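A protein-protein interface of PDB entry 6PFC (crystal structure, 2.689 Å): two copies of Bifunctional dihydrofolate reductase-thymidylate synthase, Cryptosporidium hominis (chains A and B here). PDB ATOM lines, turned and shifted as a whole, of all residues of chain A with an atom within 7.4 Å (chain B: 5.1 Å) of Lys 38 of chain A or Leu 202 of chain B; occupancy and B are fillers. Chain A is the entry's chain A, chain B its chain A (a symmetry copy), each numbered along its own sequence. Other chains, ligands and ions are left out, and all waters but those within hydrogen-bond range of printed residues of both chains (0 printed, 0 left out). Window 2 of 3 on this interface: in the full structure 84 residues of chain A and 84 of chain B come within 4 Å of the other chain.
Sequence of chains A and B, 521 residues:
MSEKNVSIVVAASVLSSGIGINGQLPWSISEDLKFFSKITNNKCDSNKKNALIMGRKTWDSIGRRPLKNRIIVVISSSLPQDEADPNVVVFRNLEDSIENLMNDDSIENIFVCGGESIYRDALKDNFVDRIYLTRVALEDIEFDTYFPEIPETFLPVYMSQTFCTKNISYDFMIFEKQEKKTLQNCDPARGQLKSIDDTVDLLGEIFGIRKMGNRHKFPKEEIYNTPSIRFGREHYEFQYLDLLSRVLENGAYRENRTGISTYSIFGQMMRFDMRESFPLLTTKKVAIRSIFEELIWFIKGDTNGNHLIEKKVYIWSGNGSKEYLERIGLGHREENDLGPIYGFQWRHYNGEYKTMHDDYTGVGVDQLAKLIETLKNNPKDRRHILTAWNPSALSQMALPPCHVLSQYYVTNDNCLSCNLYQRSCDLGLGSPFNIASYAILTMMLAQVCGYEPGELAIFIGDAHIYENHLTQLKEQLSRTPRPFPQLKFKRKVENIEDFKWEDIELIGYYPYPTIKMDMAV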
ATOM      1  N   ASP A  32      -9.223 -16.266  13.370  1.00  0.00           N
ATOM      2  CA  ASP A  32      -8.755 -14.890  13.495  1.00  0.00           C
ATOM      3  C   ASP A  32      -9.400 -14.192  14.686  1.00  0.00           C
ATOM      4  O   ASP A  32      -8.744 -13.411  15.384  1.00  0.00           O
ATOM      5  CB  ASP A  32      -9.031 -14.119  12.206  1.00  0.00           C
ATOM      6  CG  ASP A  32      -8.697 -12.647  12.326  1.00  0.00           C
ATOM      7  OD1 ASP A  32      -7.515 -12.322  12.568  1.00  0.00           O
ATOM      8  OD2 ASP A  32      -9.618 -11.815  12.177  1.00  0.00           O
ATOM      9  N   LEU A  33     -10.686 -14.459  14.933  1.00  0.00           N
ATOM     10  CA  LEU A  33     -11.340 -13.893  16.108  1.00  0.00           C
ATOM     11  C   LEU A  33     -10.734 -14.448  17.390  1.00  0.00           C
ATOM     12  O   LEU A  33     -10.568 -13.716  18.374  1.00  0.00           O
ATOM     13  CB  LEU A  33     -12.842 -14.167  16.059  1.00  0.00           C
ATOM     14  CG  LEU A  33     -13.622 -13.449  14.956  1.00  0.00           C
ATOM     15  CD1 LEU A  33     -15.108 -13.757  15.064  1.00  0.00           C
ATOM     16  CD2 LEU A  33     -13.374 -11.949  15.008  1.00  0.00           C
ATOM     17  N   LYS A  34     -10.399 -15.740  17.397  1.00  0.00           N
ATOM     18  CA  LYS A  34      -9.712 -16.317  18.547  1.00  0.00           C
ATOM     19  C   LYS A  34      -8.339 -15.684  18.734  1.00  0.00           C
ATOM     20  O   LYS A  34      -7.886 -15.489  19.868  1.00  0.00           O
ATOM     21  CB  LYS A  34      -9.590 -17.833  18.383  1.00  0.00           C
ATOM     22  N   PHE A  35      -7.665 -15.350  17.630  1.00  0.00           N
ATOM     23  CA  PHE A  35      -6.385 -14.656  17.727  1.00  0.00           C
ATOM     24  C   PHE A  35      -6.556 -13.271  18.336  1.00  0.00           C
ATOM     25  O   PHE A  35      -5.778 -12.869  19.209  1.00  0.00           O
ATOM     26  CB  PHE A  35      -5.729 -14.566  16.348  1.00  0.00           C
ATOM     27  CG  PHE A  35      -4.402 -13.854  16.349  1.00  0.00           C
ATOM     28  CD1 PHE A  35      -3.261 -14.485  16.819  1.00  0.00           C
ATOM     29  CD2 PHE A  35      -4.295 -12.558  15.871  1.00  0.00           C
ATOM     30  CE1 PHE A  35      -2.040 -13.835  16.820  1.00  0.00           C
ATOM     31  CE2 PHE A  35      -3.076 -11.902  15.868  1.00  0.00           C
ATOM     32  CZ  PHE A  35      -1.948 -12.542  16.343  1.00  0.00           C
ATOM     33  N   PHE A  36      -7.577 -12.530  17.895  1.00  0.00           N
ATOM     34  CA  PHE A  36      -7.858 -11.224  18.485  1.00  0.00           C
ATOM     35  C   PHE A  36      -8.123 -11.342  19.980  1.00  0.00           C
ATOM     36  O   PHE A  36      -7.690 -10.489  20.764  1.00  0.00           O
ATOM     37  CB  PHE A  36      -9.050 -10.575  17.780  1.00  0.00           C
ATOM     38  CG  PHE A  36      -9.486  -9.270  18.390  1.00  0.00           C
ATOM     39  CD1 PHE A  36      -8.891  -8.078  18.009  1.00  0.00           C
ATOM     40  CD2 PHE A  36     -10.496  -9.233  19.340  1.00  0.00           C
ATOM     41  CE1 PHE A  36      -9.292  -6.877  18.566  1.00  0.00           C
ATOM     42  CE2 PHE A  36     -10.898  -8.036  19.901  1.00  0.00           C
ATOM     43  CZ  PHE A  36     -10.296  -6.857  19.512  1.00  0.00           C
ATOM     44  N   SER A  37      -8.837 -12.389  20.392  1.00  0.00           N
ATOM     45  CA  SER A  37      -9.142 -12.561  21.808  1.00  0.00           C
ATOM     46  C   SER A  37      -7.879 -12.856  22.609  1.00  0.00           C
ATOM     47  O   SER A  37      -7.623 -12.219  23.638  1.00  0.00           O
ATOM     48  CB  SER A  37     -10.175 -13.676  21.987  1.00  0.00           C
ATOM     49  OG  SER A  37     -10.481 -13.882  23.355  1.00  0.00           O
ATOM     50  N   LYS A  38      -7.067 -13.808  22.144  1.00  0.00           N
ATOM     51  CA  LYS A  38      -5.885 -14.202  22.906  1.00  0.00           C
ATOM     52  C   LYS A  38      -4.805 -13.126  22.887  1.00  0.00           C
ATOM     53  O   LYS A  38      -4.056 -12.991  23.861  1.00  0.00           O
ATOM     54  CB  LYS A  38      -5.331 -15.524  22.374  1.00  0.00           C
ATOM     55  CG  LYS A  38      -6.329 -16.666  22.446  1.00  0.00           C
ATOM     56  CD  LYS A  38      -5.646 -18.018  22.506  1.00  0.00           C
ATOM     57  CE  LYS A  38      -6.656 -19.115  22.801  1.00  0.00           C
ATOM     58  NZ  LYS A  38      -6.008 -20.437  23.016  1.00  0.00           N
ATOM     59  N   ILE A  39      -4.708 -12.354  21.805  1.00  0.00           N
ATOM     60  CA  ILE A  39      -3.658 -11.343  21.744  1.00  0.00           C
ATOM     61  C   ILE A  39      -4.025 -10.120  22.581  1.00  0.00           C
ATOM     62  O   ILE A  39      -3.138  -9.424  23.086  1.00  0.00           O
ATOM     63  CB  ILE A  39      -3.357 -10.964  20.281  1.00  0.00           C
ATOM     64  CG1 ILE A  39      -1.959 -10.355  20.157  1.00  0.00           C
ATOM     65  CG2 ILE A  39      -4.397  -9.998  19.736  1.00  0.00           C
ATOM     66  CD1 ILE A  39      -0.843 -11.317  20.498  1.00  0.00           C
ATOM     67  N   THR A  40      -5.318  -9.848  22.764  1.00  0.00           N
ATOM     68  CA  THR A  40      -5.750  -8.711  23.568  1.00  0.00           C
ATOM     69  C   THR A  40      -5.954  -9.062  25.036  1.00  0.00           C
ATOM     70  O   THR A  40      -5.987  -8.156  25.875  1.00  0.00           O
ATOM     71  CB  THR A  40      -7.049  -8.116  23.007  1.00  0.00           C
ATOM     72  OG1 THR A  40      -8.043  -9.143  22.898  1.00  0.00           O
ATOM     73  CG2 THR A  40      -6.805  -7.495  21.639  1.00  0.00           C
ATOM     74  N   ASN A  41      -6.089 -10.347  25.360  1.00  0.00           N
ATOM     75  CA  ASN A  41      -6.148 -10.802  26.743  1.00  0.00           C
ATOM     76  C   ASN A  41      -4.775 -11.133  27.313  1.00  0.00           C
ATOM     77  O   ASN A  41      -4.650 -11.292  28.532  1.00  0.00           O
ATOM     78  CB  ASN A  41      -7.056 -12.033  26.861  1.00  0.00           C
ATOM     79  CG  ASN A  41      -8.524 -11.669  26.964  1.00  0.00           C
ATOM     80  OD1 ASN A  41      -8.907 -10.786  27.732  1.00  0.00           O
ATOM     81  ND2 ASN A  41      -9.359 -12.352  26.188  1.00  0.00           N
ATOM     82  N   ASN A  42      -3.752 -11.242  26.464  1.00  0.00           N
ATOM     83  CA  ASN A  42      -2.402 -11.569  26.905  1.00  0.00           C
ATOM     84  C   ASN A  42      -1.863 -10.485  27.829  1.00  0.00           C
ATOM     85  O   ASN A  42      -1.595  -9.363  27.391  1.00  0.00           O
ATOM     86  CB  ASN A  42      -1.476 -11.752  25.698  1.00  0.00           C
ATOM     87  CG  ASN A  42      -0.127 -12.337  26.078  1.00  0.00           C
ATOM     88  OD1 ASN A  42      -0.006 -13.064  27.064  1.00  0.00           O
ATOM     89  ND2 ASN A  42       0.897 -12.019  25.291  1.00  0.00           N
ATOM     90  N   LYS A  43      -1.712 -10.812  29.111  1.00  0.00           N
ATOM     91  CA  LYS A  43      -1.219  -9.867  30.100  1.00  0.00           C
ATOM     92  C   LYS A  43      -0.315 -10.597  31.082  1.00  0.00           C
ATOM     93  O   LYS A  43      -0.303 -11.829  31.156  1.00  0.00           O
ATOM     94  CB  LYS A  43      -2.373  -9.175  30.836  1.00  0.00           C
ATOM     95  CG  LYS A  43      -3.285 -10.128  31.592  1.00  0.00           C
ATOM     96  CD  LYS A  43      -4.416  -9.382  32.277  1.00  0.00           C
ATOM     97  CE  LYS A  43      -5.234 -10.311  33.155  1.00  0.00           C
ATOM     98  NZ  LYS A  43      -6.282  -9.576  33.912  1.00  0.00           N
ATOM     99  N   ASN A  50      -6.481  -5.067  30.171  1.00  0.00           N
ATOM    100  CA  ASN A  50      -6.045  -4.422  28.940  1.00  0.00           C
ATOM    101  C   ASN A  50      -7.150  -3.522  28.400  1.00  0.00           C
ATOM    102  O   ASN A  50      -8.341  -3.788  28.587  1.00  0.00           O
ATOM    103  CB  ASN A  50      -5.651  -5.457  27.882  1.00  0.00           C
ATOM    104  CG  ASN A  50      -4.339  -6.153  28.203  1.00  0.00           C
ATOM    105  OD1 ASN A  50      -3.479  -5.601  28.888  1.00  0.00           O
ATOM    106  ND2 ASN A  50      -4.176  -7.372  27.698  1.00  0.00           N
ATOM    107  N   ARG A  70     -11.701  -7.376  29.617  1.00  0.00           N
ATOM    108  CA  ARG A  70     -11.054  -6.218  29.021  1.00  0.00           C
ATOM    109  C   ARG A  70     -11.935  -4.985  29.165  1.00  0.00           C
ATOM    110  O   ARG A  70     -13.133  -5.076  29.449  1.00  0.00           O
ATOM    111  CB  ARG A  70     -10.732  -6.458  27.541  1.00  0.00           C
ATOM    112  CG  ARG A  70      -9.557  -7.391  27.306  1.00  0.00           C
ATOM    113  CD  ARG A  70      -9.722  -8.146  26.002  1.00  0.00           C
ATOM    114  NE  ARG A  70     -10.870  -9.045  26.058  1.00  0.00           N
ATOM    115  CZ  ARG A  70     -11.274  -9.806  25.048  1.00  0.00           C
ATOM    116  NH1 ARG A  70     -10.625  -9.776  23.892  1.00  0.00           N
ATOM    117  NH2 ARG A  70     -12.331 -10.596  25.194  1.00  0.00           N
ATOM    118  N   PHE A 111      -4.412  -1.566  23.204  1.00  0.00           N
ATOM    119  CA  PHE A 111      -4.584  -2.101  21.861  1.00  0.00           C
ATOM    120  C   PHE A 111      -5.494  -1.181  21.060  1.00  0.00           C
ATOM    121  O   PHE A 111      -6.529  -0.735  21.565  1.00  0.00           O
ATOM    122  CB  PHE A 111      -5.163  -3.519  21.899  1.00  0.00           C
ATOM    123  CG  PHE A 111      -4.247  -4.530  22.529  1.00  0.00           C
ATOM    124  CD1 PHE A 111      -4.235  -4.713  23.903  1.00  0.00           C
ATOM    125  CD2 PHE A 111      -3.398  -5.296  21.748  1.00  0.00           C
ATOM    126  CE1 PHE A 111      -3.392  -5.642  24.484  1.00  0.00           C
ATOM    127  CE2 PHE A 111      -2.553  -6.227  22.323  1.00  0.00           C
ATOM    128  CZ  PHE A 111      -2.550  -6.399  23.695  1.00  0.00           C
ATOM    129  N   TYR A 132      -0.044  -5.908  14.905  1.00  0.00           N
ATOM    130  CA  TYR A 132      -0.421  -7.295  14.652  1.00  0.00           C
ATOM    131  C   TYR A 132      -1.338  -7.306  13.434  1.00  0.00           C
ATOM    132  O   TYR A 132      -2.467  -6.808  13.494  1.00  0.00           O
ATOM    133  CB  TYR A 132      -1.113  -7.911  15.866  1.00  0.00           C
ATOM    134  CG  TYR A 132      -0.244  -8.029  17.099  1.00  0.00           C
ATOM    135  CD1 TYR A 132       0.560  -9.143  17.304  1.00  0.00           C
ATOM    136  CD2 TYR A 132      -0.239  -7.031  18.067  1.00  0.00           C
ATOM    137  CE1 TYR A 132       1.351  -9.258  18.434  1.00  0.00           C
ATOM    138  CE2 TYR A 132       0.549  -7.137  19.201  1.00  0.00           C
ATOM    139  CZ  TYR A 132       1.340  -8.252  19.378  1.00  0.00           C
ATOM    140  OH  TYR A 132       2.126  -8.360  20.504  1.00  0.00           O
ATOM    141  N   ASP B 198       5.519 -15.207  22.341  1.00  0.00           N
ATOM    142  CA  ASP B 198       4.145 -15.264  22.832  1.00  0.00           C
ATOM    143  C   ASP B 198       3.154 -15.460  21.691  1.00  0.00           C
ATOM    144  O   ASP B 198       2.193 -16.228  21.823  1.00  0.00           O
ATOM    145  CB  ASP B 198       3.811 -13.997  23.620  1.00  0.00           C
ATOM    146  CG  ASP B 198       4.521 -13.936  24.961  1.00  0.00           C
ATOM    147  OD1 ASP B 198       5.175 -14.932  25.337  1.00  0.00           O
ATOM    148  OD2 ASP B 198       4.418 -12.894  25.643  1.00  0.00           O
ATOM    149  N   THR B 199       3.368 -14.776  20.565  1.00  0.00           N
ATOM    150  CA  THR B 199       2.459 -14.911  19.431  1.00  0.00           C
ATOM    151  C   THR B 199       2.482 -16.329  18.870  1.00  0.00           C
ATOM    152  O   THR B 199       1.431 -16.889  18.537  1.00  0.00           O
ATOM    153  CB  THR B 199       2.815 -13.892  18.348  1.00  0.00           C
ATOM    154  OG1 THR B 199       2.669 -12.565  18.873  1.00  0.00           O
ATOM    155  CG2 THR B 199       1.906 -14.052  17.141  1.00  0.00           C
ATOM    156  N   VAL B 200       3.671 -16.926  18.760  1.00  0.00           N
ATOM    157  CA  VAL B 200       3.773 -18.296  18.266  1.00  0.00           C
ATOM    158  C   VAL B 200       3.066 -19.259  19.216  1.00  0.00           C
ATOM    159  O   VAL B 200       2.412 -20.215  18.781  1.00  0.00           O
ATOM    160  CB  VAL B 200       5.250 -18.682  18.054  1.00  0.00           C
ATOM    161  CG1 VAL B 200       5.371 -20.145  17.654  1.00  0.00           C
ATOM    162  CG2 VAL B 200       5.882 -17.793  16.996  1.00  0.00           C
ATOM    163  N   ASP B 201       3.183 -19.019  20.525  1.00  0.00           N
ATOM    164  CA  ASP B 201       2.486 -19.860  21.494  1.00  0.00           C
ATOM    165  C   ASP B 201       0.975 -19.726  21.359  1.00  0.00           C
ATOM    166  O   ASP B 201       0.248 -20.725  21.425  1.00  0.00           O
ATOM    167  CB  ASP B 201       2.927 -19.508  22.916  1.00  0.00           C
ATOM    168  CG  ASP B 201       4.354 -19.922  23.202  1.00  0.00           C
ATOM    169  OD1 ASP B 201       4.834 -20.883  22.564  1.00  0.00           O
ATOM    170  OD2 ASP B 201       4.992 -19.292  24.070  1.00  0.00           O
ATOM    171  N   LEU B 202       0.483 -18.498  21.174  1.00  0.00           N
ATOM    172  CA  LEU B 202      -0.954 -18.294  21.016  1.00  0.00           C
ATOM    173  C   LEU B 202      -1.468 -18.964  19.748  1.00  0.00           C
ATOM    174  O   LEU B 202      -2.541 -19.577  19.754  1.00  0.00           O
ATOM    175  CB  LEU B 202      -1.275 -16.800  21.005  1.00  0.00           C
ATOM    176  CG  LEU B 202      -1.022 -16.047  22.313  1.00  0.00           C
ATOM    177  CD1 LEU B 202      -1.394 -14.582  22.166  1.00  0.00           C
ATOM    178  CD2 LEU B 202      -1.796 -16.686  23.456  1.00  0.00           C
ATOM    179  N   LEU B 203      -0.716 -18.856  18.650  1.00  0.00           N
ATOM    180  CA  LEU B 203      -1.096 -19.565  17.433  1.00  0.00           C
ATOM    181  C   LEU B 203      -1.028 -21.074  17.625  1.00  0.00           C
ATOM    182  O   LEU B 203      -1.790 -21.816  16.996  1.00  0.00           O
ATOM    183  CB  LEU B 203      -0.205 -19.127  16.270  1.00  0.00           C
ATOM    184  CG  LEU B 203      -0.410 -17.693  15.778  1.00  0.00           C
ATOM    185  CD1 LEU B 203       0.571 -17.360  14.668  1.00  0.00           C
ATOM    186  CD2 LEU B 203      -1.843 -17.478  15.312  1.00  0.00           C
ATOM    187  N   GLY B 204      -0.122 -21.547  18.485  1.00  0.00           N
ATOM    188  CA  GLY B 204      -0.042 -22.966  18.788  1.00  0.00           C
ATOM    189  C   GLY B 204      -1.155 -23.470  19.682  1.00  0.00           C
ATOM    190  O   GLY B 204      -1.380 -24.683  19.749  1.00  0.00           O
ATOM    191  N   GLU B 205      -1.848 -22.570  20.379  1.00  0.00           N
ATOM    192  CA  GLU B 205      -3.016 -22.940  21.169  1.00  0.00           C
ATOM    193  C   GLU B 205      -4.289 -22.925  20.332  1.00  0.00           C
ATOM    194  O   GLU B 205      -5.147 -23.800  20.492  1.00  0.00           O
ATOM    195  CB  GLU B 205      -3.171 -21.999  22.367  1.00  0.00           C
ATOM    196  CG  GLU B 205      -2.035 -22.074  23.373  1.00  0.00           C
ATOM    197  CD  GLU B 205      -2.168 -21.048  24.484  1.00  0.00           C
ATOM    198  OE1 GLU B 205      -3.199 -20.344  24.529  1.00  0.00           O
ATOM    199  OE2 GLU B 205      -1.241 -20.948  25.316  1.00  0.00           O
ATOM    200  N   ILE B 206      -4.426 -21.935  19.448  1.00  0.00           N
ATOM    201  CA  ILE B 206      -5.572 -21.885  18.542  1.00  0.00           C
ATOM    202  C   ILE B 206      -5.550 -23.083  17.603  1.00  0.00           C
ATOM    203  O   ILE B 206      -6.437 -23.945  17.639  1.00  0.00           O
ATOM    204  CB  ILE B 206      -5.576 -20.561  17.761  1.00  0.00           C
ATOM    205  CG1 ILE B 206      -5.641 -19.377  18.726  1.00  0.00           C
ATOM    206  CG2 ILE B 206      -6.731 -20.523  16.772  1.00  0.00           C
ATOM    207  CD1 ILE B 206      -5.430 -18.050  18.058  1.00  0.00           C
ATOM    208  N   PHE B 207      -4.532 -23.157  16.753  1.00  0.00           N
ATOM    209  CA  PHE B 207      -4.346 -24.314  15.888  1.00  0.00           C
ATOM    210  C   PHE B 207      -3.626 -25.416  16.650  1.00  0.00           C
ATOM    211  O   PHE B 207      -2.627 -25.164  17.329  1.00  0.00           O
ATOM    212  CB  PHE B 207      -3.547 -23.933  14.642  1.00  0.00           C
ATOM    213  CG  PHE B 207      -4.120 -22.773  13.879  1.00  0.00           C
ATOM    214  CD1 PHE B 207      -3.701 -21.477  14.141  1.00  0.00           C
ATOM    215  CD2 PHE B 207      -5.072 -22.979  12.895  1.00  0.00           C
ATOM    216  CE1 PHE B 207      -4.227 -20.409  13.434  1.00  0.00           C
ATOM    217  CE2 PHE B 207      -5.600 -21.916  12.186  1.00  0.00           C
ATOM    218  CZ  PHE B 207      -5.176 -20.629  12.456  1.00  0.00           C
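The side-chain amino group (NZ) of Lys 38 of chain A is in salt-bridge range of the side-chain carboxylate (OE1) of Glu 205 of chain B, 3.2 Å away.
No position is printed for both chains. Of the 9 pairs that touch across the chains among the printed residues, none has its exchanged pair printed and touching as well.
Among the printed residues, pairs that only touch across the chains: Lys 34 of chain A with Ile 206 of chain B (3.8 Å), Phe 35 of chain A with Thr 199 of chain B (3.96 Å), Phe 35 of chain A with Leu 203 of chain B (3.6 Å), Phe 35 of chain A with Ile 206 of chain B (3.5 Å), Lys 38 of chain A with Leu 202 of chain B (3.5 Å), Ile 39 of chain A with Leu 202 of chain B (3.7 Å), Asn 42 of chain A with Asp 198 of chain B (3.6 Å) and Tyr 132 of chain A with Thr 199 of chain B (3.6 Å).
Printed residues of chain B within 4 Å of Lys 38 of chain A: Leu 202 (3.5 Å) and Glu 205 (3.2 Å). Of the printed residues of chain B, Asn 42 of chain A touches Asp 198 (3.6 Å). Of the printed residues of chain B, Tyr 132 of chain A touches Thr 199 (3.6 Å). Of the printed residues of chain A, Asp 198 of chain B touches Asn 42. The nearest printed residue of chain B that does not touch Lys 38 of chain A is Ile 206 of chain B (4.02 Å).
Hydrophobic or aromatic side chains of chain A within 4 Å of the printed part of chain B: Phe 35, Ile 39 and Tyr 132. Of the 10 printed residues of chain B, 6 touch a printed residue of chain A. Hydrophobic or aromatic side chains of chain B within 4 Å of the printed part of chain A: Leu 202, Leu 203 and Ile 206. Among the printed residues, 9 pairs touch across the chains. Among the printed residues, Asp or Glu carboxylates within 4 Å of a Lys or Arg side-chain nitrogen of the other chain: Lys 38 of chain A with Glu 205 of chain B.
The backbone carbonyl oxygen (O) of Asn 42 of chain A lies within hydrogen-bond range of the side-chain amide nitrogen (ND2) of Asn 50 of chain A, 3.3 Å away.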
